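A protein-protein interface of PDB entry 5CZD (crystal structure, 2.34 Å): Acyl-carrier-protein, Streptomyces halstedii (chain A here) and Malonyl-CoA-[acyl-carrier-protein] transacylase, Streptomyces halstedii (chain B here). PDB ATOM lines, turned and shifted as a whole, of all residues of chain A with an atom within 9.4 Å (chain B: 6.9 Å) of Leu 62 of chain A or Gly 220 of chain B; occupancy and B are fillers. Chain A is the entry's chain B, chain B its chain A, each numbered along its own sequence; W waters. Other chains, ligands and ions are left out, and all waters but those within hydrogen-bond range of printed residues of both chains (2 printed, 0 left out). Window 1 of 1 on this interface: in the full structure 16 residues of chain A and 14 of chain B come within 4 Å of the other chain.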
ATOM      1  N   THR A  42      -1.245  28.251 -23.757  1.00  0.00           N
ATOM      2  CA  THR A  42      -0.595  27.216 -22.983  1.00  0.00           C
ATOM      3  C   THR A  42       0.538  26.575 -23.747  1.00  0.00           C
ATOM      4  O   THR A  42       1.604  26.323 -23.199  1.00  0.00           O
ATOM      5  CB  THR A  42      -1.566  26.115 -22.542  1.00  0.00           C
ATOM      6  OG1 THR A  42      -2.677  26.692 -21.839  1.00  0.00           O
ATOM      7  CG2 THR A  42      -0.843  25.196 -21.591  1.00  0.00           C
ATOM      8  N   VAL A  43       0.306  26.300 -25.012  1.00  0.00           N
ATOM      9  CA  VAL A  43       1.338  25.729 -25.851  1.00  0.00           C
ATOM     10  C   VAL A  43       2.536  26.630 -25.922  1.00  0.00           C
ATOM     11  O   VAL A  43       3.622  26.125 -25.821  1.00  0.00           O
ATOM     12  CB  VAL A  43       0.882  25.486 -27.306  1.00  0.00           C
ATOM     13  CG1 VAL A  43       2.022  24.948 -28.147  1.00  0.00           C
ATOM     14  CG2 VAL A  43      -0.270  24.489 -27.335  1.00  0.00           C
ATOM     15  N   LEU A  45       3.364  29.084 -23.947  1.00  0.00           N
ATOM     16  CA  LEU A  45       3.883  29.142 -22.579  1.00  0.00           C
ATOM     17  C   LEU A  45       4.767  27.935 -22.186  1.00  0.00           C
ATOM     18  O   LEU A  45       5.809  28.117 -21.564  1.00  0.00           O
ATOM     19  CB  LEU A  45       2.740  29.343 -21.577  1.00  0.00           C
ATOM     20  CG  LEU A  45       3.049  29.229 -20.073  1.00  0.00           C
ATOM     21  CD1 LEU A  45       4.112  30.199 -19.566  1.00  0.00           C
ATOM     22  CD2 LEU A  45       1.764  29.453 -19.297  1.00  0.00           C
ATOM     23  N   LEU A  46       4.357  26.717 -22.524  1.00  0.00           N
ATOM     24  CA  LEU A  46       5.218  25.523 -22.364  1.00  0.00           C
ATOM     25  C   LEU A  46       6.543  25.724 -23.061  1.00  0.00           C
ATOM     26  O   LEU A  46       7.617  25.481 -22.522  1.00  0.00           O
ATOM     27  CB  LEU A  46       4.577  24.308 -23.026  1.00  0.00           C
ATOM     28  CG  LEU A  46       3.825  23.396 -22.101  1.00  0.00           C
ATOM     29  CD1 LEU A  46       2.834  22.525 -22.890  1.00  0.00           C
ATOM     30  CD2 LEU A  46       4.860  22.571 -21.349  1.00  0.00           C
ATOM     31  N   SER A  47       6.435  26.119 -24.308  1.00  0.00           N
ATOM     32  CA  SER A  47       7.595  26.461 -25.117  1.00  0.00           C
ATOM     33  C   SER A  47       8.567  27.358 -24.340  1.00  0.00           C
ATOM     34  O   SER A  47       9.692  26.965 -24.101  1.00  0.00           O
ATOM     35  CB  SER A  47       7.116  27.183 -26.387  1.00  0.00           C
ATOM     36  OG  SER A  47       7.926  26.858 -27.475  1.00  0.00           O
ATOM     37  N   GLU A  50      10.266  25.800 -21.412  1.00  0.00           N
ATOM     38  CA  GLU A  50      11.204  24.748 -21.665  1.00  0.00           C
ATOM     39  C   GLU A  50      12.536  25.307 -22.117  1.00  0.00           C
ATOM     40  O   GLU A  50      13.561  24.782 -21.711  1.00  0.00           O
ATOM     41  CB  GLU A  50      10.639  23.720 -22.635  1.00  0.00           C
ATOM     42  CG  GLU A  50       9.592  22.825 -21.948  1.00  0.00           C
ATOM     43  CD  GLU A  50       8.969  21.811 -22.890  1.00  0.00           C
ATOM     44  OE1 GLU A  50       8.906  22.119 -24.093  1.00  0.00           O
ATOM     45  OE2 GLU A  50       8.536  20.722 -22.465  1.00  0.00           O
ATOM     46  N   HIS A  56      12.128  19.637 -19.892  1.00  0.00           N
ATOM     47  CA  HIS A  56      11.164  19.005 -20.788  1.00  0.00           C
ATOM     48  C   HIS A  56       9.970  18.549 -19.957  1.00  0.00           C
ATOM     49  O   HIS A  56      10.137  17.713 -19.102  1.00  0.00           O
ATOM     50  CB  HIS A  56      11.797  17.802 -21.509  1.00  0.00           C
ATOM     51  CG  HIS A  56      10.836  17.057 -22.390  1.00  0.00           C
ATOM     52  ND1 HIS A  56      10.181  17.649 -23.455  1.00  0.00           N
ATOM     53  CD2 HIS A  56      10.398  15.774 -22.348  1.00  0.00           C
ATOM     54  CE1 HIS A  56       9.392  16.763 -24.035  1.00  0.00           C
ATOM     55  NE2 HIS A  56       9.502  15.618 -23.380  1.00  0.00           N
ATOM     56  N   PHE A  57       8.781  19.127 -20.183  1.00  0.00           N
ATOM     57  CA  PHE A  57       7.534  18.708 -19.505  1.00  0.00           C
ATOM     58  C   PHE A  57       7.042  17.368 -20.074  1.00  0.00           C
ATOM     59  O   PHE A  57       7.241  17.077 -21.232  1.00  0.00           O
ATOM     60  CB  PHE A  57       6.433  19.760 -19.684  1.00  0.00           C
ATOM     61  CG  PHE A  57       6.544  20.960 -18.768  1.00  0.00           C
ATOM     62  CD1 PHE A  57       7.559  21.900 -18.931  1.00  0.00           C
ATOM     63  CD2 PHE A  57       5.594  21.195 -17.782  1.00  0.00           C
ATOM     64  CE1 PHE A  57       7.644  23.019 -18.108  1.00  0.00           C
ATOM     65  CE2 PHE A  57       5.688  22.307 -16.939  1.00  0.00           C
ATOM     66  CZ  PHE A  57       6.717  23.218 -17.106  1.00  0.00           C
ATOM     67  N   GLN A  58       6.361  16.569 -19.265  1.00  0.00           N
ATOM     68  CA  GLN A  58       6.095  15.162 -19.604  1.00  0.00           C
ATOM     69  C   GLN A  58       5.218  14.467 -18.583  1.00  0.00           C
ATOM     70  O   GLN A  58       5.105  14.917 -17.457  1.00  0.00           O
ATOM     71  CB  GLN A  58       7.381  14.397 -19.603  1.00  0.00           C
ATOM     72  CG  GLN A  58       7.803  13.947 -20.947  1.00  0.00           C
ATOM     73  CD  GLN A  58       8.962  12.976 -20.851  1.00  0.00           C
ATOM     74  OE1 GLN A  58       9.348  12.571 -19.757  1.00  0.00           O
ATOM     75  NE2 GLN A  58       9.513  12.586 -22.004  1.00  0.00           N
ATOM     76  N   ASP A  59       4.601  13.364 -19.000  1.00  0.00           N
ATOM     77  CA  ASP A  59       3.763  12.536 -18.128  1.00  0.00           C
ATOM     78  C   ASP A  59       2.771  13.455 -17.432  1.00  0.00           C
ATOM     79  O   ASP A  59       2.070  14.199 -18.137  1.00  0.00           O
ATOM     80  CB  ASP A  59       4.655  11.733 -17.182  1.00  0.00           C
ATOM     81  CG  ASP A  59       5.568  10.778 -17.929  1.00  0.00           C
ATOM     82  OD1 ASP A  59       5.094  10.126 -18.872  1.00  0.00           O
ATOM     83  OD2 ASP A  59       6.763  10.697 -17.595  1.00  0.00           O
ATOM     84  N   GLU A  60       2.759  13.519 -16.100  1.00  0.00           N
ATOM     85  CA  GLU A  60       1.694  14.264 -15.418  1.00  0.00           C
ATOM     86  C   GLU A  60       1.805  15.775 -15.586  1.00  0.00           C
ATOM     87  O   GLU A  60       0.799  16.493 -15.497  1.00  0.00           O
ATOM     88  CB  GLU A  60       1.579  13.887 -13.933  1.00  0.00           C
ATOM     89  CG  GLU A  60       1.049  12.473 -13.717  1.00  0.00           C
ATOM     90  CD  GLU A  60       2.054  11.404 -14.168  1.00  0.00           C
ATOM     91  OE1 GLU A  60       3.281  11.627 -13.961  1.00  0.00           O
ATOM     92  OE2 GLU A  60       1.629  10.368 -14.751  1.00  0.00           O
ATOM     93  N   ALA A  61       2.999  16.265 -15.867  1.00  0.00           N
ATOM     94  CA  ALA A  61       3.167  17.701 -16.097  1.00  0.00           C
ATOM     95  C   ALA A  61       2.427  18.221 -17.364  1.00  0.00           C
ATOM     96  O   ALA A  61       2.232  19.427 -17.532  1.00  0.00           O
ATOM     97  CB  ALA A  61       4.662  18.062 -16.153  1.00  0.00           C
ATOM     98  N   LEU A  62       2.020  17.321 -18.249  1.00  0.00           N
ATOM     99  CA  LEU A  62       1.214  17.734 -19.410  1.00  0.00           C
ATOM    100  C   LEU A  62      -0.322  17.684 -19.269  1.00  0.00           C
ATOM    101  O   LEU A  62      -1.042  18.034 -20.195  1.00  0.00           O
ATOM    102  CB  LEU A  62       1.636  16.943 -20.628  1.00  0.00           C
ATOM    103  CG  LEU A  62       3.026  17.310 -21.098  1.00  0.00           C
ATOM    104  CD1 LEU A  62       3.424  16.413 -22.251  1.00  0.00           C
ATOM    105  CD2 LEU A  62       3.141  18.799 -21.461  1.00  0.00           C
ATOM    106  N   THR A  63      -0.831  17.282 -18.118  1.00  0.00           N
ATOM    107  CA  THR A  63      -2.269  17.346 -17.883  1.00  0.00           C
ATOM    108  C   THR A  63      -2.678  18.806 -17.747  1.00  0.00           C
ATOM    109  O   THR A  63      -1.864  19.672 -17.431  1.00  0.00           O
ATOM    110  CB  THR A  63      -2.638  16.622 -16.587  1.00  0.00           C
ATOM    111  OG1 THR A  63      -1.906  17.202 -15.517  1.00  0.00           O
ATOM    112  CG2 THR A  63      -2.279  15.131 -16.643  1.00  0.00           C
ATOM    113  N   LYS A  64      -3.952  19.075 -17.975  1.00  0.00           N
ATOM    114  CA  LYS A  64      -4.506  20.414 -17.824  1.00  0.00           C
ATOM    115  C   LYS A  64      -4.349  20.940 -16.397  1.00  0.00           C
ATOM    116  O   LYS A  64      -4.429  22.153 -16.140  1.00  0.00           O
ATOM    117  CB  LYS A  64      -6.000  20.398 -18.175  1.00  0.00           C
ATOM    118  CG  LYS A  64      -6.328  20.148 -19.650  1.00  0.00           C
ATOM    119  CD  LYS A  64      -5.803  21.249 -20.589  1.00  0.00           C
ATOM    120  CE  LYS A  64      -6.459  21.198 -21.957  1.00  0.00           C
ATOM    121  NZ  LYS A  64      -5.931  22.270 -22.843  1.00  0.00           N
ATOM    122  N   GLU A  65      -4.168  20.020 -15.458  1.00  0.00           N
ATOM    123  CA  GLU A  65      -4.208  20.382 -14.055  1.00  0.00           C
ATOM    124  C   GLU A  65      -2.993  21.247 -13.699  1.00  0.00           C
ATOM    125  O   GLU A  65      -3.102  22.198 -12.918  1.00  0.00           O
ATOM    126  CB  GLU A  65      -4.301  19.126 -13.174  1.00  0.00           C
ATOM    127  CG  GLU A  65      -5.716  18.545 -13.100  1.00  0.00           C
ATOM    128  CD  GLU A  65      -6.240  17.935 -14.410  1.00  0.00           C
ATOM    129  OE1 GLU A  65      -5.454  17.576 -15.327  1.00  0.00           O
ATOM    130  OE2 GLU A  65      -7.476  17.793 -14.524  1.00  0.00           O
ATOM    131  N   THR A  66      -1.855  20.886 -14.284  1.00  0.00           N
ATOM    132  CA  THR A  66      -0.586  21.606 -14.158  1.00  0.00           C
ATOM    133  C   THR A  66      -0.792  23.093 -14.386  1.00  0.00           C
ATOM    134  O   THR A  66      -0.210  23.914 -13.682  1.00  0.00           O
ATOM    135  CB  THR A  66       0.433  21.105 -15.188  1.00  0.00           C
ATOM    136  OG1 THR A  66       0.614  19.694 -15.036  1.00  0.00           O
ATOM    137  CG2 THR A  66       1.772  21.796 -15.021  1.00  0.00           C
ATOM    138  N   PHE A  67      -1.682  23.409 -15.327  1.00  0.00           N
ATOM    139  CA  PHE A  67      -1.891  24.766 -15.797  1.00  0.00           C
ATOM    140  C   PHE A  67      -3.082  25.493 -15.177  1.00  0.00           C
ATOM    141  O   PHE A  67      -3.400  26.618 -15.573  1.00  0.00           O
ATOM    142  CB  PHE A  67      -1.991  24.725 -17.312  1.00  0.00           C
ATOM    143  CG  PHE A  67      -0.721  24.203 -17.986  1.00  0.00           C
ATOM    144  CD1 PHE A  67      -0.644  22.898 -18.449  1.00  0.00           C
ATOM    145  CD2 PHE A  67       0.399  25.031 -18.130  1.00  0.00           C
ATOM    146  CE1 PHE A  67       0.524  22.429 -19.034  1.00  0.00           C
ATOM    147  CE2 PHE A  67       1.569  24.564 -18.716  1.00  0.00           C
ATOM    148  CZ  PHE A  67       1.639  23.266 -19.170  1.00  0.00           C
ATOM    149  N   LEU A  73       1.422  25.463 -11.181  1.00  0.00           N
ATOM    150  CA  LEU A  73       2.407  25.496 -12.261  1.00  0.00           C
ATOM    151  C   LEU A  73       3.812  25.767 -11.710  1.00  0.00           C
ATOM    152  O   LEU A  73       4.782  25.120 -12.126  1.00  0.00           O
ATOM    153  CB  LEU A  73       1.997  26.537 -13.297  1.00  0.00           C
ATOM    154  CG  LEU A  73       2.933  26.777 -14.466  1.00  0.00           C
ATOM    155  CD1 LEU A  73       3.071  25.521 -15.287  1.00  0.00           C
ATOM    156  CD2 LEU A  73       2.440  27.921 -15.318  1.00  0.00           C
ATOM    157  N   THR A  76       4.967  22.677  -9.925  1.00  0.00           N
ATOM    158  CA  THR A  76       5.297  21.601 -10.855  1.00  0.00           C
ATOM    159  C   THR A  76       6.638  21.863 -11.553  1.00  0.00           C
ATOM    160  O   THR A  76       7.422  20.945 -11.828  1.00  0.00           O
ATOM    161  CB  THR A  76       4.147  21.379 -11.843  1.00  0.00           C
ATOM    162  OG1 THR A  76       2.955  21.098 -11.095  1.00  0.00           O
ATOM    163  CG2 THR A  76       4.463  20.219 -12.803  1.00  0.00           C
ATOM    164  N   MET A  80      11.904  20.385 -11.302  1.00  0.00           N
ATOM    165  CA  MET A  80      12.790  20.016 -12.398  1.00  0.00           C
ATOM    166  C   MET A  80      14.022  20.943 -12.426  1.00  0.00           C
ATOM    167  O   MET A  80      13.935  22.154 -12.151  1.00  0.00           O
ATOM    168  CB  MET A  80      11.999  20.092 -13.710  1.00  0.00           C
ATOM    169  CG  MET A  80      10.766  19.172 -13.801  1.00  0.00           C
ATOM    170  SD  MET A  80       9.471  19.712 -14.961  1.00  0.00           S
ATOM    171  CE  MET A  80       8.849  18.139 -15.557  1.00  0.00           C
ATOM    172  N   VAL B 168      -0.889  18.391 -29.568  1.00  0.00           N
ATOM    173  CA  VAL B 168       0.263  19.172 -30.045  1.00  0.00           C
ATOM    174  C   VAL B 168       1.563  18.568 -29.553  1.00  0.00           C
ATOM    175  O   VAL B 168       1.540  17.727 -28.704  1.00  0.00           O
ATOM    176  CB  VAL B 168       0.204  20.639 -29.537  1.00  0.00           C
ATOM    177  CG1 VAL B 168      -0.843  21.432 -30.288  1.00  0.00           C
ATOM    178  CG2 VAL B 168      -0.070  20.692 -28.038  1.00  0.00           C
ATOM    179  N   ARG B 169       2.690  19.045 -30.069  1.00  0.00           N
ATOM    180  CA  ARG B 169       4.031  18.632 -29.632  1.00  0.00           C
ATOM    181  C   ARG B 169       4.201  17.173 -29.965  1.00  0.00           C
ATOM    182  O   ARG B 169       4.848  16.446 -29.235  1.00  0.00           O
ATOM    183  CB  ARG B 169       4.261  18.887 -28.138  1.00  0.00           C
ATOM    184  CG  ARG B 169       4.188  20.365 -27.742  1.00  0.00           C
ATOM    185  CD  ARG B 169       4.000  20.600 -26.248  1.00  0.00           C
ATOM    186  NE  ARG B 169       4.806  19.737 -25.393  1.00  0.00           N
ATOM    187  CZ  ARG B 169       5.933  20.082 -24.764  1.00  0.00           C
ATOM    188  NH1 ARG B 169       6.554  19.201 -24.005  1.00  0.00           N
ATOM    189  NH2 ARG B 169       6.456  21.296 -24.885  1.00  0.00           N
ATOM    190  N   ALA B 170       3.621  16.775 -31.096  1.00  0.00           N
ATOM    191  CA  ALA B 170       3.553  15.385 -31.560  1.00  0.00           C
ATOM    192  C   ALA B 170       4.040  15.242 -33.001  1.00  0.00           C
ATOM    193  O   ALA B 170       3.227  15.296 -33.942  1.00  0.00           O
ATOM    194  CB  ALA B 170       2.121  14.903 -31.479  1.00  0.00           C
ATOM    195  N   ARG B 215      -0.686   8.171 -23.227  1.00  0.00           N
ATOM    196  CA  ARG B 215       0.389   7.768 -24.107  1.00  0.00           C
ATOM    197  C   ARG B 215       1.013   8.981 -24.857  1.00  0.00           C
ATOM    198  O   ARG B 215       2.235   9.096 -24.977  1.00  0.00           O
ATOM    199  CB  ARG B 215      -0.164   6.740 -25.080  1.00  0.00           C
ATOM    200  CG  ARG B 215       0.796   6.324 -26.178  1.00  0.00           C
ATOM    201  CD  ARG B 215       1.943   5.425 -25.716  1.00  0.00           C
ATOM    202  NE  ARG B 215       2.669   4.945 -26.908  1.00  0.00           N
ATOM    203  CZ  ARG B 215       3.539   5.682 -27.597  1.00  0.00           C
ATOM    204  NH1 ARG B 215       3.805   6.929 -27.223  1.00  0.00           N
ATOM    205  NH2 ARG B 215       4.125   5.193 -28.677  1.00  0.00           N
ATOM    206  N   LEU B 216       0.171   9.872 -25.360  1.00  0.00           N
ATOM    207  CA  LEU B 216       0.638  11.169 -25.845  1.00  0.00           C
ATOM    208  C   LEU B 216       1.621  11.816 -24.881  1.00  0.00           C
ATOM    209  O   LEU B 216       2.770  11.987 -25.240  1.00  0.00           O
ATOM    210  CB  LEU B 216      -0.534  12.119 -26.079  1.00  0.00           C
ATOM    211  CG  LEU B 216      -1.322  11.818 -27.339  1.00  0.00           C
ATOM    212  CD1 LEU B 216      -2.605  12.595 -27.322  1.00  0.00           C
ATOM    213  CD2 LEU B 216      -0.477  12.151 -28.551  1.00  0.00           C
ATOM    214  N   ARG B 217       1.161  12.123 -23.665  1.00  0.00           N
ATOM    215  CA  ARG B 217       1.996  12.715 -22.590  1.00  0.00           C
ATOM    216  C   ARG B 217       3.320  11.995 -22.268  1.00  0.00           C
ATOM    217  O   ARG B 217       4.299  12.644 -21.857  1.00  0.00           O
ATOM    218  CB  ARG B 217       1.234  12.799 -21.290  1.00  0.00           C
ATOM    219  CG  ARG B 217      -0.021  13.645 -21.282  1.00  0.00           C
ATOM    220  CD  ARG B 217      -0.529  13.722 -19.863  1.00  0.00           C
ATOM    221  NE  ARG B 217      -1.958  13.444 -19.731  1.00  0.00           N
ATOM    222  CZ  ARG B 217      -2.496  12.396 -19.101  1.00  0.00           C
ATOM    223  NH1 ARG B 217      -1.773  11.427 -18.530  1.00  0.00           N
ATOM    224  NH2 ARG B 217      -3.793  12.317 -19.056  1.00  0.00           N
ATOM    225  N   SER B 218       3.323  10.673 -22.426  1.00  0.00           N
ATOM    226  CA  SER B 218       4.524   9.857 -22.236  1.00  0.00           C
ATOM    227  C   SER B 218       5.685  10.301 -23.086  1.00  0.00           C
ATOM    228  O   SER B 218       6.820  10.164 -22.695  1.00  0.00           O
ATOM    229  CB  SER B 218       4.245   8.390 -22.578  1.00  0.00           C
ATOM    230  OG  SER B 218       3.224   7.903 -21.732  1.00  0.00           O
ATOM    231  N   VAL B 219       5.392  10.770 -24.275  1.00  0.00           N
ATOM    232  CA  VAL B 219       6.417  11.148 -25.243  1.00  0.00           C
ATOM    233  C   VAL B 219       6.463  12.686 -25.425  1.00  0.00           C
ATOM    234  O   VAL B 219       7.012  13.162 -26.377  1.00  0.00           O
ATOM    235  CB  VAL B 219       6.185  10.439 -26.587  1.00  0.00           C
ATOM    236  CG1 VAL B 219       6.366   8.927 -26.448  1.00  0.00           C
ATOM    237  CG2 VAL B 219       4.789  10.731 -27.124  1.00  0.00           C
ATOM    238  N   GLY B 220       5.865  13.430 -24.501  1.00  0.00           N
ATOM    239  CA  GLY B 220       5.956  14.891 -24.464  1.00  0.00           C
ATOM    240  C   GLY B 220       4.862  15.605 -25.239  1.00  0.00           C
ATOM    241  O   GLY B 220       4.856  16.839 -25.301  1.00  0.00           O
ATOM    242  N   ALA B 221       3.929  14.832 -25.816  1.00  0.00           N
ATOM    243  CA  ALA B 221       2.817  15.381 -26.582  1.00  0.00           C
ATOM    244  C   ALA B 221       1.761  15.847 -25.611  1.00  0.00           C
ATOM    245  O   ALA B 221       1.649  15.298 -24.523  1.00  0.00           O
ATOM    246  CB  ALA B 221       2.268  14.353 -27.572  1.00  0.00           C
ATOM    247  N   MET B 222       1.007  16.885 -25.956  1.00  0.00           N
ATOM    248  CA  MET B 222       0.033  17.441 -25.011  1.00  0.00           C
ATOM    249  C   MET B 222      -1.370  17.351 -25.539  1.00  0.00           C
ATOM    250  O   MET B 222      -1.646  17.941 -26.558  1.00  0.00           O
ATOM    251  CB  MET B 222       0.334  18.907 -24.688  1.00  0.00           C
ATOM    252  CG  MET B 222      -0.372  19.380 -23.422  1.00  0.00           C
ATOM    253  SD  MET B 222      -0.311  21.158 -23.207  1.00  0.00           S
ATOM    254  CE  MET B 222      -1.351  21.261 -21.767  1.00  0.00           C
ATOM    255  N   PRO B 223      -2.274  16.629 -24.842  1.00  0.00           N
ATOM    256  CA  PRO B 223      -3.675  16.599 -25.300  1.00  0.00           C
ATOM    257  C   PRO B 223      -4.342  17.963 -25.167  1.00  0.00           C
ATOM    258  O   PRO B 223      -4.127  18.672 -24.150  1.00  0.00           O
ATOM    259  CB  PRO B 223      -4.319  15.598 -24.342  1.00  0.00           C
ATOM    260  CG  PRO B 223      -3.197  14.678 -24.020  1.00  0.00           C
ATOM    261  CD  PRO B 223      -2.048  15.606 -23.805  1.00  0.00           C
HETATM  262  O   HOH W   1       2.012   9.217 -19.211  1.00  0.00           O
HETATM  263  O   HOH W   2       0.581  11.275 -17.594  1.00  0.00           O
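O of Val 168 of chain B lies within hydrogen-bond range of N of Met 222 of chain B (2.9 Å).
NE of Arg 169 of chain B lies within hydrogen-bond range of O of Gly 220 of chain B (2.9 Å).
The backbone NH (N) of Ala 221 of chain B sits at hydrogen-bond distance from the backbone carbonyl oxygen (O) of Leu 216 of chain B (3.1 Å).
The side-chain carboxylate (OE2) of Glu 50 of chain A is in hydrogen-bond range of the backbone NH (N) of Phe 57 of chain A (2.8 Å).
The side-chain amide nitrogen (NE2) of Gln 58 of chain A sits close to a ring nitrogen (NE2) of His 56 of chain A, at 3.3 Å.
The backbone carbonyl oxygen (O) of Glu 60 of chain A sits at hydrogen-bond distance from the side-chain hydroxyl (OG1) of Thr 63 of chain A, 2.8 Å away.
NH2 of Arg 169 of chain B is in salt-bridge range of OE1 of Glu 50 of chain A (2.7 Å).
The backbone carbonyl oxygen (O) of Arg 217 of chain B lies within hydrogen-bond range of the backbone NH (N) of Asp 59 of chain A (3.0 Å).
Hydrophobic or aromatic side chains of chain B within 4 Å of the printed part of chain A: Val 168 and Met 222.
Of the 21 printed residues of chain A, 11 touch a printed residue of chain B.
Hydrophobic or aromatic side chains of chain A within 4 Å of the printed part of chain B: Val 43, Leu 46, His 56, Leu 62 and Phe 67.
Leu 45 of chain A touches none of the printed residues of chain B.
Printed residues of chain B within 4 Å of Glu 50 of chain A: Arg 169.
Of the printed residues of chain B, His 56 of chain A touches Arg 169 (3.7 Å) and Gly 220 (3.8 Å).
Of the printed residues of chain B, Asp 59 of chain A touches Arg 217 and Ser 218.
Leu 62 of chain A touches just these residues of chain B: Arg 217, Gly 220, Ala 221 and Met 222.
Printed residues of chain B within 4 Å of Phe 67 of chain A: Met 222 (3.5 Å).
Leu 216 of chain B touches none of the printed residues of chain A.
Printed residues of chain A within 4 Å of Arg 217 of chain B: Gln 58 (3.8 Å), Asp 59 (3.0 Å), Leu 62 (3.7 Å) and Thr 63 (3.5 Å).
Val 219 of chain B touches none of the printed residues of chain A.
Printed residues of chain A within 4 Å of Gly 220 of chain B: His 56 and Leu 62.
Of chain A, only Leu 62 comes within 4 Å of Ala 221 of chain B.
The nearest residue of chain B that does not touch Leu 62 of chain A is Arg 169 of chain B (4.3 Å).
The nearest printed residue of chain A that does not touch Gly 220 of chain B is Gln 58 of chain A (4.1 Å).
The nearest printed residue of chain B that does not touch Glu 50 of chain A is Gly 220 of chain B (6.1 Å).
Water W2 lies within hydrogen-bond range of NH1 of Arg 217 of chain B, OE2 of Glu 60 of chain A and O of Asp 59 of chain A.
Water W1 bridges OG of Ser 218 of chain B (3.1 Å) and OD1 of Asp 59 of chain A (3.2 Å).
Thr 42 of chain A touches Met 222 of chain B.
His 56 of chain A touches Arg 169 of chain B (CE1 to NH1, 3.7 Å).
Gly 220 of chain B touches His 56 of chain A (CA to NE2, 3.8 Å).
Gln 58 of chain A touches Ser 218 of chain B (NE2 to O, 3.7 Å).
CA of Ser 218 of chain B touches OD1 of Asp 59 of chain A, 3.4 Å away.
Arg 217 of chain B touches Leu 62 of chain A.
Leu 62 of chain A touches Gly 220 of chain B.
Leu 62 of chain A touches Met 222 of chain B (O to CG, 3.6 Å).
Arg 217 of chain B touches Thr 63 of chain A.
Met 222 of chain B touches Phe 67 of chain A (CE to CE1, 3.5 Å).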
